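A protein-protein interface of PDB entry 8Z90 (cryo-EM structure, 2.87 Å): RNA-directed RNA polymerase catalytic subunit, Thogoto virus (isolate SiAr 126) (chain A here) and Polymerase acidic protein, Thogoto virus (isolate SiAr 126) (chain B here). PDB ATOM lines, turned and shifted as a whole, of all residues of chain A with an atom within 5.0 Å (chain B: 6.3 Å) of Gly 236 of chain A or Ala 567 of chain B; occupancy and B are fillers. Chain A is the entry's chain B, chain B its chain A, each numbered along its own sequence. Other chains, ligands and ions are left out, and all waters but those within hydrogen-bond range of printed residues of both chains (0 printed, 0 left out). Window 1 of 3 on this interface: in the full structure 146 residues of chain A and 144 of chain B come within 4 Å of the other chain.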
ATOM      1  N   GLU A 234      -9.554  34.921  35.375  1.00  0.00           N
ATOM      2  CA  GLU A 234     -10.306  34.187  34.367  1.00  0.00           C
ATOM      3  C   GLU A 234      -9.362  33.316  33.552  1.00  0.00           C
ATOM      4  O   GLU A 234      -8.318  33.779  33.083  1.00  0.00           O
ATOM      5  CB  GLU A 234     -11.078  35.130  33.444  1.00  0.00           C
ATOM      6  CG  GLU A 234     -11.533  34.481  32.144  1.00  0.00           C
ATOM      7  CD  GLU A 234     -12.882  33.802  32.261  1.00  0.00           C
ATOM      8  OE1 GLU A 234     -13.315  33.163  31.280  1.00  0.00           O
ATOM      9  OE2 GLU A 234     -13.497  33.884  33.341  1.00  0.00           O
ATOM     10  N   ARG A 235      -9.737  32.052  33.387  1.00  0.00           N
ATOM     11  CA  ARG A 235      -8.907  31.064  32.719  1.00  0.00           C
ATOM     12  C   ARG A 235      -9.582  30.609  31.434  1.00  0.00           C
ATOM     13  O   ARG A 235     -10.776  30.294  31.426  1.00  0.00           O
ATOM     14  CB  ARG A 235      -8.655  29.862  33.633  1.00  0.00           C
ATOM     15  CG  ARG A 235      -7.713  30.159  34.784  1.00  0.00           C
ATOM     16  CD  ARG A 235      -7.511  28.937  35.656  1.00  0.00           C
ATOM     17  NE  ARG A 235      -6.465  29.141  36.649  1.00  0.00           N
ATOM     18  CZ  ARG A 235      -5.176  28.920  36.435  1.00  0.00           C
ATOM     19  NH1 ARG A 235      -4.734  28.492  35.266  1.00  0.00           N
ATOM     20  NH2 ARG A 235      -4.309  29.136  37.420  1.00  0.00           N
ATOM     21  N   GLY A 236      -8.814  30.578  30.350  1.00  0.00           N
ATOM     22  CA  GLY A 236      -9.305  30.108  29.075  1.00  0.00           C
ATOM     23  C   GLY A 236      -9.487  31.157  28.001  1.00  0.00           C
ATOM     24  O   GLY A 236     -10.060  30.844  26.951  1.00  0.00           O
ATOM     25  N   ARG A 237      -9.033  32.389  28.217  1.00  0.00           N
ATOM     26  CA  ARG A 237      -9.125  33.413  27.189  1.00  0.00           C
ATOM     27  C   ARG A 237      -7.818  34.186  27.119  1.00  0.00           C
ATOM     28  O   ARG A 237      -7.129  34.369  28.125  1.00  0.00           O
ATOM     29  CB  ARG A 237     -10.274  34.395  27.441  1.00  0.00           C
ATOM     30  CG  ARG A 237     -11.657  33.775  27.498  1.00  0.00           C
ATOM     31  CD  ARG A 237     -12.698  34.872  27.585  1.00  0.00           C
ATOM     32  NE  ARG A 237     -12.818  35.572  26.311  1.00  0.00           N
ATOM     33  CZ  ARG A 237     -12.400  36.809  26.085  1.00  0.00           C
ATOM     34  NH1 ARG A 237     -11.739  37.493  27.004  1.00  0.00           N
ATOM     35  NH2 ARG A 237     -12.627  37.364  24.898  1.00  0.00           N
ATOM     36  N   LEU A 238      -7.488  34.643  25.911  1.00  0.00           N
ATOM     37  CA  LEU A 238      -6.315  35.481  25.702  1.00  0.00           C
ATOM     38  C   LEU A 238      -6.535  36.919  26.150  1.00  0.00           C
ATOM     39  O   LEU A 238      -5.607  37.548  26.669  1.00  0.00           O
ATOM     40  CB  LEU A 238      -5.912  35.457  24.224  1.00  0.00           C
ATOM     41  CG  LEU A 238      -4.911  36.507  23.737  1.00  0.00           C
ATOM     42  CD1 LEU A 238      -3.499  36.144  24.164  1.00  0.00           C
ATOM     43  CD2 LEU A 238      -4.996  36.669  22.229  1.00  0.00           C
ATOM     44  N   PRO B 560      -1.837  34.341  29.541  1.00  0.00           N
ATOM     45  CA  PRO B 560      -3.037  34.422  28.692  1.00  0.00           C
ATOM     46  C   PRO B 560      -2.880  33.738  27.347  1.00  0.00           C
ATOM     47  O   PRO B 560      -3.855  33.161  26.849  1.00  0.00           O
ATOM     48  CB  PRO B 560      -3.257  35.932  28.535  1.00  0.00           C
ATOM     49  CG  PRO B 560      -2.628  36.517  29.741  1.00  0.00           C
ATOM     50  CD  PRO B 560      -1.428  35.675  30.016  1.00  0.00           C
ATOM     51  N   MET B 562      -1.047  30.969  26.747  1.00  0.00           N
ATOM     52  CA  MET B 562      -1.215  29.545  27.018  1.00  0.00           C
ATOM     53  C   MET B 562      -2.666  29.197  27.318  1.00  0.00           C
ATOM     54  O   MET B 562      -3.172  28.182  26.825  1.00  0.00           O
ATOM     55  CB  MET B 562      -0.323  29.120  28.182  1.00  0.00           C
ATOM     56  CG  MET B 562      -0.545  27.691  28.648  1.00  0.00           C
ATOM     57  SD  MET B 562       0.380  26.485  27.681  1.00  0.00           S
ATOM     58  CE  MET B 562       2.044  27.106  27.893  1.00  0.00           C
ATOM     59  N   GLU B 563      -3.344  30.020  28.119  1.00  0.00           N
ATOM     60  CA  GLU B 563      -4.738  29.754  28.453  1.00  0.00           C
ATOM     61  C   GLU B 563      -5.613  29.763  27.206  1.00  0.00           C
ATOM     62  O   GLU B 563      -6.420  28.851  26.995  1.00  0.00           O
ATOM     63  CB  GLU B 563      -5.238  30.781  29.470  1.00  0.00           C
ATOM     64  CG  GLU B 563      -4.661  30.631  30.874  1.00  0.00           C
ATOM     65  CD  GLU B 563      -5.221  29.446  31.648  1.00  0.00           C
ATOM     66  OE1 GLU B 563      -5.773  28.509  31.032  1.00  0.00           O
ATOM     67  OE2 GLU B 563      -5.107  29.453  32.891  1.00  0.00           O
ATOM     68  N   GLY B 564      -5.455  30.784  26.359  1.00  0.00           N
ATOM     69  CA  GLY B 564      -6.245  30.847  25.141  1.00  0.00           C
ATOM     70  C   GLY B 564      -5.937  29.711  24.186  1.00  0.00           C
ATOM     71  O   GLY B 564      -6.849  29.114  23.605  1.00  0.00           O
ATOM     72  N   PHE B 565      -4.651  29.392  24.014  1.00  0.00           N
ATOM     73  CA  PHE B 565      -4.262  28.283  23.151  1.00  0.00           C
ATOM     74  C   PHE B 565      -4.896  26.983  23.620  1.00  0.00           C
ATOM     75  O   PHE B 565      -5.527  26.268  22.834  1.00  0.00           O
ATOM     76  CB  PHE B 565      -2.737  28.165  23.121  1.00  0.00           C
ATOM     77  CG  PHE B 565      -2.231  26.938  22.415  1.00  0.00           C
ATOM     78  CD1 PHE B 565      -2.112  26.913  21.037  1.00  0.00           C
ATOM     79  CD2 PHE B 565      -1.861  25.813  23.132  1.00  0.00           C
ATOM     80  CE1 PHE B 565      -1.643  25.788  20.388  1.00  0.00           C
ATOM     81  CE2 PHE B 565      -1.394  24.685  22.489  1.00  0.00           C
ATOM     82  CZ  PHE B 565      -1.284  24.673  21.116  1.00  0.00           C
ATOM     83  N   LEU B 566      -4.755  26.668  24.908  1.00  0.00           N
ATOM     84  CA  LEU B 566      -5.298  25.419  25.426  1.00  0.00           C
ATOM     85  C   LEU B 566      -6.819  25.388  25.350  1.00  0.00           C
ATOM     86  O   LEU B 566      -7.396  24.347  25.023  1.00  0.00           O
ATOM     87  CB  LEU B 566      -4.829  25.202  26.861  1.00  0.00           C
ATOM     88  CG  LEU B 566      -3.374  24.755  27.007  1.00  0.00           C
ATOM     89  CD1 LEU B 566      -3.004  24.619  28.471  1.00  0.00           C
ATOM     90  CD2 LEU B 566      -3.133  23.451  26.265  1.00  0.00           C
ATOM     91  N   ALA B 567      -7.484  26.509  25.643  1.00  0.00           N
ATOM     92  CA  ALA B 567      -8.940  26.526  25.611  1.00  0.00           C
ATOM     93  C   ALA B 567      -9.484  26.368  24.199  1.00  0.00           C
ATOM     94  O   ALA B 567     -10.460  25.637  23.994  1.00  0.00           O
ATOM     95  CB  ALA B 567      -9.463  27.817  26.235  1.00  0.00           C
ATOM     96  N   ASN B 568      -8.878  27.032  23.217  1.00  0.00           N
ATOM     97  CA  ASN B 568      -9.348  26.965  21.843  1.00  0.00           C
ATOM     98  C   ASN B 568      -8.810  25.758  21.091  1.00  0.00           C
ATOM     99  O   ASN B 568      -9.263  25.489  19.974  1.00  0.00           O
ATOM    100  CB  ASN B 568      -8.972  28.249  21.098  1.00  0.00           C
ATOM    101  CG  ASN B 568      -9.666  29.470  21.660  1.00  0.00           C
ATOM    102  OD1 ASN B 568     -10.861  29.672  21.447  1.00  0.00           O
ATOM    103  ND2 ASN B 568      -8.921  30.292  22.387  1.00  0.00           N
ATOM    104  N   MET B 569      -7.868  25.020  21.674  1.00  0.00           N
ATOM    105  CA  MET B 569      -7.231  23.905  20.998  1.00  0.00           C
ATOM    106  C   MET B 569      -7.881  22.566  21.333  1.00  0.00           C
ATOM    107  O   MET B 569      -7.699  21.591  20.590  1.00  0.00           O
ATOM    108  CB  MET B 569      -5.742  23.897  21.376  1.00  0.00           C
ATOM    109  CG  MET B 569      -4.930  22.758  20.846  1.00  0.00           C
ATOM    110  SD  MET B 569      -4.626  23.071  19.104  1.00  0.00           S
ATOM    111  CE  MET B 569      -3.989  21.490  18.608  1.00  0.00           C
ATOM    112  N   ARG B 570      -8.650  22.506  22.421  1.00  0.00           N
ATOM    113  CA  ARG B 570      -9.385  21.298  22.773  1.00  0.00           C
ATOM    114  C   ARG B 570     -10.419  20.934  21.716  1.00  0.00           C
ATOM    115  O   ARG B 570     -10.677  19.747  21.495  1.00  0.00           O
ATOM    116  CB  ARG B 570     -10.055  21.483  24.134  1.00  0.00           C
ATOM    117  CG  ARG B 570      -9.062  21.648  25.268  1.00  0.00           C
ATOM    118  CD  ARG B 570      -9.715  21.538  26.628  1.00  0.00           C
ATOM    119  NE  ARG B 570     -10.334  22.798  27.020  1.00  0.00           N
ATOM    120  CZ  ARG B 570      -9.784  23.675  27.847  1.00  0.00           C
ATOM    121  NH1 ARG B 570      -8.588  23.473  28.373  1.00  0.00           N
ATOM    122  NH2 ARG B 570     -10.449  24.786  28.151  1.00  0.00           N
ATOM    123  N   ARG B 571     -11.010  21.932  21.057  1.00  0.00           N
ATOM    124  CA  ARG B 571     -11.930  21.657  19.958  1.00  0.00           C
ATOM    125  C   ARG B 571     -11.228  20.926  18.821  1.00  0.00           C
ATOM    126  O   ARG B 571     -11.751  19.941  18.289  1.00  0.00           O
ATOM    127  CB  ARG B 571     -12.538  22.962  19.454  1.00  0.00           C
ATOM    128  CG  ARG B 571     -13.866  23.318  20.084  1.00  0.00           C
ATOM    129  CD  ARG B 571     -14.431  24.572  19.451  1.00  0.00           C
ATOM    130  NE  ARG B 571     -13.562  25.720  19.677  1.00  0.00           N
ATOM    131  CZ  ARG B 571     -13.564  26.454  20.781  1.00  0.00           C
ATOM    132  NH1 ARG B 571     -14.378  26.187  21.788  1.00  0.00           N
ATOM    133  NH2 ARG B 571     -12.727  27.482  20.876  1.00  0.00           N
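The side-chain carboxylate (OE2) of Glu 563 of chain B is in salt-bridge range of the guanidinium group (NH1) of Arg 235 of chain A, 2.6 Å away.
Gly 236 of chain A touches Glu 563 of chain B.
CB of Ala 567 of chain B touches O of Gly 236 of chain A, 3.2 Å away.
Arg 237 of chain A touches Pro 560 of chain B.
Leu 238 of chain A touches Pro 560 of chain B (O to CB, 3.4 Å).
Of chain A, only Gly 236 comes within 4 Å of Ala 567 of chain B.
Of the printed residues of chain A, Glu 563 of chain B touches Arg 235 and Gly 236.
Of the printed residues of chain A, Pro 560 of chain B touches Arg 237 (3.7 Å) and Leu 238 (3.4 Å).
Arg 570 of chain B touches none of the printed residues of chain A.
The nearest printed residue of chain A that does not touch Glu 563 of chain B is Arg 237 of chain A (4.3 Å).
Of the 5 printed residues of chain A, 4 touch a printed residue of chain B.
Printed residues of chain A that touch a printed residue of chain B: Arg 235, Gly 236, Arg 237 and Leu 238.
Of the 11 printed residues of chain B, 3 touch a printed residue of chain A.
Hydrophobic or aromatic side chains of chain B within 4 Å of the printed part of chain A: Pro 560 and Ala 567.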
